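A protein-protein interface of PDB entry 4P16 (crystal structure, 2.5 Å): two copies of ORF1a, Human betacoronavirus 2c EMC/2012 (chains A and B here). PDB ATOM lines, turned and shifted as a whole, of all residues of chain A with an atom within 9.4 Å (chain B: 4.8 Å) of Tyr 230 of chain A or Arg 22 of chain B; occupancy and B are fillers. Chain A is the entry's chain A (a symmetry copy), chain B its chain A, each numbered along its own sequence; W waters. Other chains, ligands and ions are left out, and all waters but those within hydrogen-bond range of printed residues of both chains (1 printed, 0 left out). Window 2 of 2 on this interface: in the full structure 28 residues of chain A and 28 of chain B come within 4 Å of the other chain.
The backbone NH (N) of Val 12 of chain B lies within hydrogen-bond range of the backbone carbonyl oxygen (O) of Val 24 of chain B, 2.8 Å away. The guanidinium group of Arg 22 of chain B is in salt-bridge range of the side-chain carboxylate of Glu 70 of chain B, at 2.9 Å. The side-chain carboxylate (OE1) of Glu 70 of chain B lies within hydrogen-bond range of the backbone NH (N) of Thr 67 of chain B (2.9 Å). N of Lys 203 of chain A is in hydrogen-bond range of O of Glu 195 of chain A (2.8 Å). The side-chain hydroxyl (OH) of Tyr 215 of chain A lies within hydrogen-bond range of the guanidinium group (NH2) of Arg 240 of chain A (3.2 Å). O of Tyr 230 of chain A sits at hydrogen-bond distance from N of Arg 238 of chain A (2.8 Å).
The backbone carbonyl oxygen of Thr 23 of chain B is in hydrogen-bond range of the backbone NH of Val 231 of chain A, 2.9 Å away. The side-chain amide oxygen (OD1) of Asn 65 of chain B is in hydrogen-bond range of the side-chain hydroxyl (OH) of Tyr 215 of chain A (2.9 Å).
Glu 195 of chain A touches Thr 67 of chain B. CD1 of Tyr 230 of chain A touches NH1 of Arg 22 of chain B, at 3.4 Å. Tyr 230 of chain A touches Thr 23 of chain B (CB to O, 3.3 Å). CB of Tyr 230 of chain A touches CG2 of Val 24 of chain B, 3.8 Å away. OH of Tyr 230 of chain A touches CG2 of Thr 67 of chain B, 3.7 Å away.
No position is printed for both chains.
Water W1 lies within hydrogen-bond range of the side-chain carboxylate (OE2) of Glu 195 of chain A (2.7 Å) and the side-chain hydroxyl (OG1) of Thr 67 of chain B (3.2 Å).
Hydrophobic or aromatic side chains of chain B within 4 Å of the printed part of chain A: Val 24. Hydrophobic or aromatic side chains of chain A within 4 Å of the printed part of chain B: Tyr 215, Tyr 230 and Val 231. Among the printed residues, no Asp or Glu carboxylate lies within 4 Å of a Lys or Arg side-chain nitrogen of the other chain.
Trp 196 of chain A touches none of the printed residues of chain B. Of the printed residues of chain B, Tyr 215 of chain A touches Asn 65. No residue of chain A comes within 4 Å of Val 14 of chain B. Asn 20 of chain B touches none of the printed residues of chain A. Of chain A, only Tyr 230 comes within 4 Å of Arg 22 of chain B. Of chain A, only Tyr 230 (3.3 Å) and Val 231 (2.9 Å) come within 4 Å of Thr 23 of chain B. Of the printed residues of chain A, Val 24 of chain B touches Tyr 230 (3.8 Å). The nearest residue of chain A that does not touch Arg 22 of chain B is Val 231 of chain A (5.3 Å). The nearest printed residue of chain B that does not touch Glu 195 of chain A is Glu 70 of chain B (6.7 Å).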
ATOM      1  N   ARG A 194     -19.829  -7.712  27.091  1.00  0.00           N
ATOM      2  CA  ARG A 194     -19.364  -6.486  27.702  1.00  0.00           C
ATOM      3  C   ARG A 194     -18.085  -6.094  27.016  1.00  0.00           C
ATOM      4  O   ARG A 194     -17.178  -6.923  26.837  1.00  0.00           O
ATOM      5  CB  ARG A 194     -19.165  -6.650  29.214  1.00  0.00           C
ATOM      6  CG  ARG A 194     -18.577  -5.434  29.921  1.00  0.00           C
ATOM      7  CD  ARG A 194     -18.757  -5.545  31.414  1.00  0.00           C
ATOM      8  NE  ARG A 194     -20.172  -5.491  31.792  1.00  0.00           N
ATOM      9  CZ  ARG A 194     -20.711  -6.196  32.782  1.00  0.00           C
ATOM     10  NH1 ARG A 194     -19.958  -7.015  33.511  1.00  0.00           N
ATOM     11  NH2 ARG A 194     -22.006  -6.093  33.048  1.00  0.00           N
ATOM     12  N   GLU A 195     -18.039  -4.823  26.598  1.00  0.00           N
ATOM     13  CA  GLU A 195     -16.892  -4.173  25.964  1.00  0.00           C
ATOM     14  C   GLU A 195     -16.461  -3.071  26.911  1.00  0.00           C
ATOM     15  O   GLU A 195     -17.302  -2.269  27.318  1.00  0.00           O
ATOM     16  CB  GLU A 195     -17.285  -3.612  24.605  1.00  0.00           C
ATOM     17  CG  GLU A 195     -17.338  -4.686  23.536  1.00  0.00           C
ATOM     18  CD  GLU A 195     -17.224  -4.210  22.101  1.00  0.00           C
ATOM     19  OE1 GLU A 195     -17.109  -5.077  21.204  1.00  0.00           O
ATOM     20  OE2 GLU A 195     -17.213  -2.977  21.873  1.00  0.00           O
ATOM     21  N   TRP A 196     -15.186  -3.063  27.337  1.00  0.00           N
ATOM     22  CA  TRP A 196     -14.751  -2.063  28.316  1.00  0.00           C
ATOM     23  C   TRP A 196     -13.272  -1.704  28.307  1.00  0.00           C
ATOM     24  O   TRP A 196     -12.411  -2.477  27.885  1.00  0.00           O
ATOM     25  CB  TRP A 196     -15.154  -2.504  29.753  1.00  0.00           C
ATOM     26  CG  TRP A 196     -14.224  -3.497  30.395  1.00  0.00           C
ATOM     27  CD1 TRP A 196     -13.239  -3.232  31.302  1.00  0.00           C
ATOM     28  CD2 TRP A 196     -14.157  -4.913  30.134  1.00  0.00           C
ATOM     29  NE1 TRP A 196     -12.567  -4.390  31.624  1.00  0.00           N
ATOM     30  CE2 TRP A 196     -13.136  -5.442  30.954  1.00  0.00           C
ATOM     31  CE3 TRP A 196     -14.902  -5.797  29.325  1.00  0.00           C
ATOM     32  CZ2 TRP A 196     -12.842  -6.812  30.997  1.00  0.00           C
ATOM     33  CZ3 TRP A 196     -14.587  -7.151  29.342  1.00  0.00           C
ATOM     34  CH2 TRP A 196     -13.564  -7.647  30.164  1.00  0.00           C
ATOM     35  N   CYS A 197     -13.011  -0.509  28.837  1.00  0.00           N
ATOM     36  CA  CYS A 197     -11.723   0.065  29.160  1.00  0.00           C
ATOM     37  C   CYS A 197     -11.878   0.513  30.600  1.00  0.00           C
ATOM     38  O   CYS A 197     -12.840   1.212  30.916  1.00  0.00           O
ATOM     39  CB  CYS A 197     -11.383   1.249  28.258  1.00  0.00           C
ATOM     40  SG  CYS A 197      -9.908   2.180  28.783  1.00  0.00           S
ATOM     41  N   LYS A 203     -19.535  -0.750  28.087  1.00  0.00           N
ATOM     42  CA  LYS A 203     -20.633  -0.815  27.126  1.00  0.00           C
ATOM     43  C   LYS A 203     -21.136  -2.261  27.066  1.00  0.00           C
ATOM     44  O   LYS A 203     -20.353  -3.192  26.865  1.00  0.00           O
ATOM     45  CB  LYS A 203     -20.203  -0.324  25.726  1.00  0.00           C
ATOM     46  CG  LYS A 203     -20.793   1.021  25.325  1.00  0.00           C
ATOM     47  CD  LYS A 203     -20.395   1.411  23.895  1.00  0.00           C
ATOM     48  CE  LYS A 203     -19.166   2.298  23.815  1.00  0.00           C
ATOM     49  NZ  LYS A 203     -19.023   2.934  22.476  1.00  0.00           N
ATOM     50  N   VAL A 205     -23.756  -4.999  25.279  1.00  0.00           N
ATOM     51  CA  VAL A 205     -24.464  -5.288  24.032  1.00  0.00           C
ATOM     52  C   VAL A 205     -25.286  -6.534  24.309  1.00  0.00           C
ATOM     53  O   VAL A 205     -24.716  -7.540  24.731  1.00  0.00           O
ATOM     54  CB  VAL A 205     -23.516  -5.472  22.813  1.00  0.00           C
ATOM     55  CG1 VAL A 205     -24.133  -4.875  21.568  1.00  0.00           C
ATOM     56  CG2 VAL A 205     -22.123  -4.880  23.073  1.00  0.00           C
ATOM     57  N   TYR A 215     -23.168 -18.705  17.388  1.00  0.00           N
ATOM     58  CA  TYR A 215     -21.920 -17.965  17.304  1.00  0.00           C
ATOM     59  C   TYR A 215     -21.033 -18.543  16.249  1.00  0.00           C
ATOM     60  O   TYR A 215     -20.837 -19.744  16.196  1.00  0.00           O
ATOM     61  CB  TYR A 215     -21.180 -17.915  18.642  1.00  0.00           C
ATOM     62  CG  TYR A 215     -20.126 -16.837  18.712  1.00  0.00           C
ATOM     63  CD1 TYR A 215     -20.455 -15.535  19.086  1.00  0.00           C
ATOM     64  CD2 TYR A 215     -18.795 -17.115  18.416  1.00  0.00           C
ATOM     65  CE1 TYR A 215     -19.492 -14.529  19.132  1.00  0.00           C
ATOM     66  CE2 TYR A 215     -17.820 -16.116  18.463  1.00  0.00           C
ATOM     67  CZ  TYR A 215     -18.175 -14.824  18.824  1.00  0.00           C
ATOM     68  OH  TYR A 215     -17.225 -13.833  18.873  1.00  0.00           O
ATOM     69  N   ARG A 227     -11.516 -13.809  27.376  1.00  0.00           N
ATOM     70  CA  ARG A 227     -11.401 -12.360  27.273  1.00  0.00           C
ATOM     71  C   ARG A 227     -10.570 -11.992  26.046  1.00  0.00           C
ATOM     72  O   ARG A 227      -9.492 -12.548  25.821  1.00  0.00           O
ATOM     73  CB  ARG A 227     -10.802 -11.742  28.545  1.00  0.00           C
ATOM     74  CG  ARG A 227     -10.913 -10.211  28.573  1.00  0.00           C
ATOM     75  CD  ARG A 227     -10.177  -9.569  29.728  1.00  0.00           C
ATOM     76  NE  ARG A 227      -8.784 -10.014  29.845  1.00  0.00           N
ATOM     77  CZ  ARG A 227      -8.336 -10.826  30.800  1.00  0.00           C
ATOM     78  NH1 ARG A 227      -9.161 -11.282  31.734  1.00  0.00           N
ATOM     79  NH2 ARG A 227      -7.063 -11.193  30.824  1.00  0.00           N
ATOM     80  N   MET A 228     -11.097 -11.065  25.250  1.00  0.00           N
ATOM     81  CA  MET A 228     -10.433 -10.549  24.062  1.00  0.00           C
ATOM     82  C   MET A 228      -9.880  -9.200  24.443  1.00  0.00           C
ATOM     83  O   MET A 228     -10.562  -8.457  25.147  1.00  0.00           O
ATOM     84  CB  MET A 228     -11.434 -10.427  22.901  1.00  0.00           C
ATOM     85  CG  MET A 228     -12.060 -11.759  22.487  1.00  0.00           C
ATOM     86  SD  MET A 228     -11.173 -12.476  21.079  1.00  0.00           S
ATOM     87  CE  MET A 228      -9.798 -13.401  21.950  1.00  0.00           C
ATOM     88  N   THR A 229      -8.643  -8.894  24.026  1.00  0.00           N
ATOM     89  CA  THR A 229      -7.964  -7.635  24.351  1.00  0.00           C
ATOM     90  C   THR A 229      -7.348  -6.985  23.071  1.00  0.00           C
ATOM     91  O   THR A 229      -6.778  -7.664  22.226  1.00  0.00           O
ATOM     92  CB  THR A 229      -6.933  -7.841  25.543  1.00  0.00           C
ATOM     93  OG1 THR A 229      -7.554  -8.492  26.673  1.00  0.00           O
ATOM     94  CG2 THR A 229      -6.291  -6.523  26.034  1.00  0.00           C
ATOM     95  N   TYR A 230      -7.500  -5.677  22.932  1.00  0.00           N
ATOM     96  CA  TYR A 230      -6.924  -4.894  21.830  1.00  0.00           C
ATOM     97  C   TYR A 230      -6.680  -3.449  22.332  1.00  0.00           C
ATOM     98  O   TYR A 230      -7.052  -3.138  23.470  1.00  0.00           O
ATOM     99  CB  TYR A 230      -7.765  -4.971  20.514  1.00  0.00           C
ATOM    100  CG  TYR A 230      -9.201  -4.523  20.651  1.00  0.00           C
ATOM    101  CD1 TYR A 230     -10.184  -5.397  21.104  1.00  0.00           C
ATOM    102  CD2 TYR A 230      -9.579  -3.218  20.344  1.00  0.00           C
ATOM    103  CE1 TYR A 230     -11.512  -4.989  21.245  1.00  0.00           C
ATOM    104  CE2 TYR A 230     -10.906  -2.795  20.482  1.00  0.00           C
ATOM    105  CZ  TYR A 230     -11.869  -3.687  20.932  1.00  0.00           C
ATOM    106  OH  TYR A 230     -13.174  -3.290  21.101  1.00  0.00           O
ATOM    107  N   VAL A 231      -6.019  -2.600  21.519  1.00  0.00           N
ATOM    108  CA  VAL A 231      -5.687  -1.219  21.883  1.00  0.00           C
ATOM    109  C   VAL A 231      -6.953  -0.326  21.983  1.00  0.00           C
ATOM    110  O   VAL A 231      -7.771  -0.323  21.056  1.00  0.00           O
ATOM    111  CB  VAL A 231      -4.637  -0.652  20.873  1.00  0.00           C
ATOM    112  CG1 VAL A 231      -4.475   0.863  21.002  1.00  0.00           C
ATOM    113  CG2 VAL A 231      -3.290  -1.350  21.011  1.00  0.00           C
ATOM    114  N   CYS A 232      -7.098   0.440  23.093  1.00  0.00           N
ATOM    115  CA  CYS A 232      -8.193   1.411  23.267  1.00  0.00           C
ATOM    116  C   CYS A 232      -7.774   2.762  22.662  1.00  0.00           C
ATOM    117  O   CYS A 232      -6.566   3.037  22.538  1.00  0.00           O
ATOM    118  CB  CYS A 232      -8.575   1.578  24.737  1.00  0.00           C
ATOM    119  SG  CYS A 232     -10.095   2.542  25.001  1.00  0.00           S
ATOM    120  N   GLN A 233      -8.770   3.621  22.322  1.00  0.00           N
ATOM    121  CA  GLN A 233      -8.509   4.969  21.808  1.00  0.00           C
ATOM    122  C   GLN A 233      -7.646   5.799  22.777  1.00  0.00           C
ATOM    123  O   GLN A 233      -6.704   6.436  22.334  1.00  0.00           O
ATOM    124  CB  GLN A 233      -9.798   5.701  21.434  1.00  0.00           C
ATOM    125  CG  GLN A 233     -10.791   5.918  22.569  1.00  0.00           C
ATOM    126  CD  GLN A 233     -10.895   7.386  22.882  1.00  0.00           C
ATOM    127  OE1 GLN A 233     -11.635   8.127  22.226  1.00  0.00           O
ATOM    128  NE2 GLN A 233     -10.125   7.846  23.862  1.00  0.00           N
ATOM    129  N   CYS A 234      -7.901   5.693  24.093  1.00  0.00           N
ATOM    130  CA  CYS A 234      -7.179   6.372  25.165  1.00  0.00           C
ATOM    131  C   CYS A 234      -5.683   6.048  25.194  1.00  0.00           C
ATOM    132  O   CYS A 234      -4.908   6.829  25.741  1.00  0.00           O
ATOM    133  CB  CYS A 234      -7.831   6.062  26.508  1.00  0.00           C
ATOM    134  SG  CYS A 234      -7.459   4.407  27.142  1.00  0.00           S
ATOM    135  N   GLY A 235      -5.310   4.892  24.653  1.00  0.00           N
ATOM    136  CA  GLY A 235      -3.939   4.395  24.605  1.00  0.00           C
ATOM    137  C   GLY A 235      -3.717   3.155  25.453  1.00  0.00           C
ATOM    138  O   GLY A 235      -2.665   2.511  25.361  1.00  0.00           O
ATOM    139  N   GLY A 236      -4.705   2.828  26.291  1.00  0.00           N
ATOM    140  CA  GLY A 236      -4.647   1.675  27.172  1.00  0.00           C
ATOM    141  C   GLY A 236      -5.111   0.419  26.475  1.00  0.00           C
ATOM    142  O   GLY A 236      -4.962   0.272  25.249  1.00  0.00           O
ATOM    143  N   GLU A 237      -5.656  -0.508  27.269  1.00  0.00           N
ATOM    144  CA  GLU A 237      -6.198  -1.765  26.762  1.00  0.00           C
ATOM    145  C   GLU A 237      -7.725  -1.720  26.791  1.00  0.00           C
ATOM    146  O   GLU A 237      -8.316  -1.140  27.712  1.00  0.00           O
ATOM    147  CB  GLU A 237      -5.671  -2.956  27.565  1.00  0.00           C
ATOM    148  CG  GLU A 237      -4.212  -3.280  27.312  1.00  0.00           C
ATOM    149  CD  GLU A 237      -3.650  -4.377  28.202  1.00  0.00           C
ATOM    150  OE1 GLU A 237      -2.987  -5.292  27.665  1.00  0.00           O
ATOM    151  OE2 GLU A 237      -3.861  -4.322  29.435  1.00  0.00           O
ATOM    152  N   ARG A 238      -8.348  -2.295  25.755  1.00  0.00           N
ATOM    153  CA  ARG A 238      -9.799  -2.431  25.558  1.00  0.00           C
ATOM    154  C   ARG A 238     -10.077  -3.940  25.543  1.00  0.00           C
ATOM    155  O   ARG A 238      -9.316  -4.714  24.938  1.00  0.00           O
ATOM    156  CB  ARG A 238     -10.227  -1.785  24.212  1.00  0.00           C
ATOM    157  CG  ARG A 238     -11.723  -1.733  23.958  1.00  0.00           C
ATOM    158  CD  ARG A 238     -12.235  -0.322  23.803  1.00  0.00           C
ATOM    159  NE  ARG A 238     -13.675  -0.256  24.048  1.00  0.00           N
ATOM    160  CZ  ARG A 238     -14.269   0.618  24.859  1.00  0.00           C
ATOM    161  NH1 ARG A 238     -15.590   0.604  25.007  1.00  0.00           N
ATOM    162  NH2 ARG A 238     -13.548   1.523  25.522  1.00  0.00           N
ATOM    163  N   HIS A 239     -11.135  -4.356  26.238  1.00  0.00           N
ATOM    164  CA  HIS A 239     -11.487  -5.771  26.316  1.00  0.00           C
ATOM    165  C   HIS A 239     -12.906  -6.034  25.856  1.00  0.00           C
ATOM    166  O   HIS A 239     -13.775  -5.161  25.968  1.00  0.00           O
ATOM    167  CB  HIS A 239     -11.331  -6.331  27.747  1.00  0.00           C
ATOM    168  CG  HIS A 239     -10.146  -5.836  28.502  1.00  0.00           C
ATOM    169  ND1 HIS A 239      -8.913  -6.458  28.398  1.00  0.00           N
ATOM    170  CD2 HIS A 239     -10.045  -4.794  29.357  1.00  0.00           C
ATOM    171  CE1 HIS A 239      -8.096  -5.761  29.167  1.00  0.00           C
ATOM    172  NE2 HIS A 239      -8.727  -4.739  29.747  1.00  0.00           N
ATOM    173  N   ARG A 240     -13.140  -7.268  25.390  1.00  0.00           N
ATOM    174  CA  ARG A 240     -14.447  -7.776  25.005  1.00  0.00           C
ATOM    175  C   ARG A 240     -14.568  -9.132  25.655  1.00  0.00           C
ATOM    176  O   ARG A 240     -13.677  -9.971  25.494  1.00  0.00           O
ATOM    177  CB  ARG A 240     -14.585  -7.878  23.469  1.00  0.00           C
ATOM    178  CG  ARG A 240     -15.958  -8.368  22.998  1.00  0.00           C
ATOM    179  CD  ARG A 240     -16.103  -8.187  21.503  1.00  0.00           C
ATOM    180  NE  ARG A 240     -16.459  -9.430  20.821  1.00  0.00           N
ATOM    181  CZ  ARG A 240     -17.686  -9.731  20.422  1.00  0.00           C
ATOM    182  NH1 ARG A 240     -18.694  -8.889  20.645  1.00  0.00           N
ATOM    183  NH2 ARG A 240     -17.921 -10.877  19.795  1.00  0.00           N
ATOM    184  N   GLN A 241     -15.644  -9.346  26.420  1.00  0.00           N
ATOM    185  CA  GLN A 241     -15.866 -10.614  27.103  1.00  0.00           C
ATOM    186  C   GLN A 241     -17.365 -10.882  27.285  1.00  0.00           C
ATOM    187  O   GLN A 241     -18.117  -9.952  27.589  1.00  0.00           O
ATOM    188  CB  GLN A 241     -15.144 -10.624  28.468  1.00  0.00           C
ATOM    189  CG  GLN A 241     -14.742 -12.022  28.970  1.00  0.00           C
ATOM    190  CD  GLN A 241     -14.482 -12.110  30.461  1.00  0.00           C
ATOM    191  OE1 GLN A 241     -14.752 -11.187  31.242  1.00  0.00           O
ATOM    192  NE2 GLN A 241     -14.032 -13.271  30.909  1.00  0.00           N
ATOM    193  N   VAL B  12      -0.774  -5.246  14.842  1.00  0.00           N
ATOM    194  CA  VAL B  12      -1.474  -5.445  13.578  1.00  0.00           C
ATOM    195  C   VAL B  12      -2.720  -4.528  13.562  1.00  0.00           C
ATOM    196  O   VAL B  12      -3.265  -4.208  14.627  1.00  0.00           O
ATOM    197  CB  VAL B  12      -1.764  -6.963  13.445  1.00  0.00           C
ATOM    198  CG1 VAL B  12      -3.234  -7.323  13.668  1.00  0.00           C
ATOM    199  CG2 VAL B  12      -1.193  -7.544  12.164  1.00  0.00           C
ATOM    200  N   LEU B  13      -3.131  -4.074  12.377  1.00  0.00           N
ATOM    201  CA  LEU B  13      -4.295  -3.215  12.251  1.00  0.00           C
ATOM    202  C   LEU B  13      -5.434  -3.997  11.645  1.00  0.00           C
ATOM    203  O   LEU B  13      -5.287  -4.583  10.573  1.00  0.00           O
ATOM    204  CB  LEU B  13      -3.967  -1.965  11.439  1.00  0.00           C
ATOM    205  CG  LEU B  13      -3.082  -0.944  12.167  1.00  0.00           C
ATOM    206  CD1 LEU B  13      -2.084  -0.305  11.210  1.00  0.00           C
ATOM    207  CD2 LEU B  13      -3.912   0.064  12.968  1.00  0.00           C
ATOM    208  N   VAL B  14      -6.562  -4.049  12.354  1.00  0.00           N
ATOM    209  CA  VAL B  14      -7.716  -4.848  11.964  1.00  0.00           C
ATOM    210  C   VAL B  14      -8.870  -3.985  11.449  1.00  0.00           C
ATOM    211  O   VAL B  14      -9.268  -3.023  12.111  1.00  0.00           O
ATOM    212  CB  VAL B  14      -8.119  -5.784  13.133  1.00  0.00           C
ATOM    213  CG1 VAL B  14      -9.378  -6.563  12.827  1.00  0.00           C
ATOM    214  CG2 VAL B  14      -6.991  -6.746  13.471  1.00  0.00           C
ATOM    215  N   ASN B  20     -12.245   2.180   8.963  1.00  0.00           N
ATOM    216  CA  ASN B  20     -11.981   2.126  10.402  1.00  0.00           C
ATOM    217  C   ASN B  20     -11.042   0.970  10.717  1.00  0.00           C
ATOM    218  O   ASN B  20     -11.223  -0.124  10.185  1.00  0.00           O
ATOM    219  CB  ASN B  20     -13.291   1.995  11.185  1.00  0.00           C
ATOM    220  CG  ASN B  20     -14.345   2.979  10.727  1.00  0.00           C
ATOM    221  OD1 ASN B  20     -14.480   4.089  11.262  1.00  0.00           O
ATOM    222  ND2 ASN B  20     -15.088   2.615   9.683  1.00  0.00           N
ATOM    223  N   PHE B  21     -10.020   1.225  11.562  1.00  0.00           N
ATOM    224  CA  PHE B  21      -8.986   0.251  11.941  1.00  0.00           C
ATOM    225  C   PHE B  21      -8.757   0.185  13.453  1.00  0.00           C
ATOM    226  O   PHE B  21      -8.710   1.239  14.099  1.00  0.00           O
ATOM    227  CB  PHE B  21      -7.634   0.588  11.249  1.00  0.00           C
ATOM    228  CG  PHE B  21      -7.619   0.438   9.746  1.00  0.00           C
ATOM    229  CD1 PHE B  21      -8.152   1.422   8.929  1.00  0.00           C
ATOM    230  CD2 PHE B  21      -6.984  -0.644   9.145  1.00  0.00           C
ATOM    231  CE1 PHE B  21      -8.131   1.288   7.538  1.00  0.00           C
ATOM    232  CE2 PHE B  21      -7.009  -0.808   7.757  1.00  0.00           C
ATOM    233  CZ  PHE B  21      -7.579   0.166   6.961  1.00  0.00           C
ATOM    234  N   ARG B  22      -8.570  -1.045  14.011  1.00  0.00           N
ATOM    235  CA  ARG B  22      -8.233  -1.236  15.438  1.00  0.00           C
ATOM    236  C   ARG B  22      -6.936  -1.942  15.567  1.00  0.00           C
ATOM    237  O   ARG B  22      -6.662  -2.848  14.791  1.00  0.00           O
ATOM    238  CB  ARG B  22      -9.323  -1.955  16.263  1.00  0.00           C
ATOM    239  CG  ARG B  22      -9.464  -3.446  16.025  1.00  0.00           C
ATOM    240  CD  ARG B  22     -10.679  -3.921  16.732  1.00  0.00           C
ATOM    241  NE  ARG B  22     -11.151  -5.206  16.233  1.00  0.00           N
ATOM    242  CZ  ARG B  22     -10.911  -6.378  16.806  1.00  0.00           C
ATOM    243  NH1 ARG B  22     -10.120  -6.456  17.872  1.00  0.00           N
ATOM    244  NH2 ARG B  22     -11.455  -7.486  16.314  1.00  0.00           N
ATOM    245  N   THR B  23      -6.115  -1.518  16.521  1.00  0.00           N
ATOM    246  CA  THR B  23      -4.815  -2.131  16.752  1.00  0.00           C
ATOM    247  C   THR B  23      -4.956  -3.283  17.707  1.00  0.00           C
ATOM    248  O   THR B  23      -5.642  -3.191  18.737  1.00  0.00           O
ATOM    249  CB  THR B  23      -3.779  -1.115  17.199  1.00  0.00           C
ATOM    250  OG1 THR B  23      -3.937   0.048  16.410  1.00  0.00           O
ATOM    251  CG2 THR B  23      -2.357  -1.617  17.029  1.00  0.00           C
ATOM    252  N   VAL B  24      -4.320  -4.391  17.329  1.00  0.00           N
ATOM    253  CA  VAL B  24      -4.292  -5.619  18.109  1.00  0.00           C
ATOM    254  C   VAL B  24      -2.817  -5.994  18.250  1.00  0.00           C
ATOM    255  O   VAL B  24      -2.075  -5.982  17.256  1.00  0.00           O
ATOM    256  CB  VAL B  24      -5.122  -6.736  17.429  1.00  0.00           C
ATOM    257  CG1 VAL B  24      -5.074  -8.040  18.229  1.00  0.00           C
ATOM    258  CG2 VAL B  24      -6.570  -6.294  17.193  1.00  0.00           C
ATOM    259  N   LEU B  36      -7.038 -14.055  17.462  1.00  0.00           N
ATOM    260  CA  LEU B  36      -7.929 -13.027  16.950  1.00  0.00           C
ATOM    261  C   LEU B  36      -9.165 -13.591  16.198  1.00  0.00           C
ATOM    262  O   LEU B  36     -10.303 -13.301  16.593  1.00  0.00           O
ATOM    263  CB  LEU B  36      -7.080 -12.096  16.088  1.00  0.00           C
ATOM    264  CG  LEU B  36      -7.738 -10.907  15.443  1.00  0.00           C
ATOM    265  CD1 LEU B  36      -8.270  -9.920  16.508  1.00  0.00           C
ATOM    266  CD2 LEU B  36      -6.764 -10.244  14.487  1.00  0.00           C
ATOM    267  N   LEU B  62     -10.512  -9.003   8.991  1.00  0.00           N
ATOM    268  CA  LEU B  62     -11.167  -9.964   9.867  1.00  0.00           C
ATOM    269  C   LEU B  62     -12.533 -10.324   9.275  1.00  0.00           C
ATOM    270  O   LEU B  62     -13.158  -9.458   8.680  1.00  0.00           O
ATOM    271  CB  LEU B  62     -11.309  -9.335  11.270  1.00  0.00           C
ATOM    272  CG  LEU B  62     -11.784 -10.202  12.428  1.00  0.00           C
ATOM    273  CD1 LEU B  62     -10.723 -11.152  12.872  1.00  0.00           C
ATOM    274  CD2 LEU B  62     -12.146  -9.351  13.614  1.00  0.00           C
ATOM    275  N   ASN B  65     -15.625 -13.073  14.834  1.00  0.00           N
ATOM    276  CA  ASN B  65     -15.204 -12.555  16.160  1.00  0.00           C
ATOM    277  C   ASN B  65     -15.039 -11.028  16.132  1.00  0.00           C
ATOM    278  O   ASN B  65     -14.106 -10.505  16.736  1.00  0.00           O
ATOM    279  CB  ASN B  65     -13.916 -13.219  16.670  1.00  0.00           C
ATOM    280  CG  ASN B  65     -14.064 -14.694  16.940  1.00  0.00           C
ATOM    281  OD1 ASN B  65     -14.858 -15.122  17.790  1.00  0.00           O
ATOM    282  ND2 ASN B  65     -13.285 -15.501  16.225  1.00  0.00           N
ATOM    283  N   THR B  67     -15.922  -6.975  16.723  1.00  0.00           N
ATOM    284  CA  THR B  67     -16.363  -6.138  17.850  1.00  0.00           C
ATOM    285  C   THR B  67     -17.757  -5.601  17.514  1.00  0.00           C
ATOM    286  O   THR B  67     -18.169  -5.685  16.352  1.00  0.00           O
ATOM    287  CB  THR B  67     -15.402  -4.961  18.062  1.00  0.00           C
ATOM    288  OG1 THR B  67     -15.548  -4.023  16.985  1.00  0.00           O
ATOM    289  CG2 THR B  67     -13.967  -5.400  18.223  1.00  0.00           C
ATOM    290  N   GLU B  70     -17.469  -3.107  14.808  1.00  0.00           N
ATOM    291  CA  GLU B  70     -17.194  -3.782  13.535  1.00  0.00           C
ATOM    292  C   GLU B  70     -18.475  -4.397  12.973  1.00  0.00           C
ATOM    293  O   GLU B  70     -18.739  -4.253  11.774  1.00  0.00           O
ATOM    294  CB  GLU B  70     -16.106  -4.841  13.696  1.00  0.00           C
ATOM    295  CG  GLU B  70     -14.700  -4.332  13.443  1.00  0.00           C
ATOM    296  CD  GLU B  70     -13.577  -5.148  14.062  1.00  0.00           C
ATOM    297  OE1 GLU B  70     -13.864  -5.987  14.946  1.00  0.00           O
ATOM    298  OE2 GLU B  70     -12.403  -4.927  13.684  1.00  0.00           O
HETATM  299  O   HOH W   1     -16.916  -2.344  19.309  1.00  0.00           O
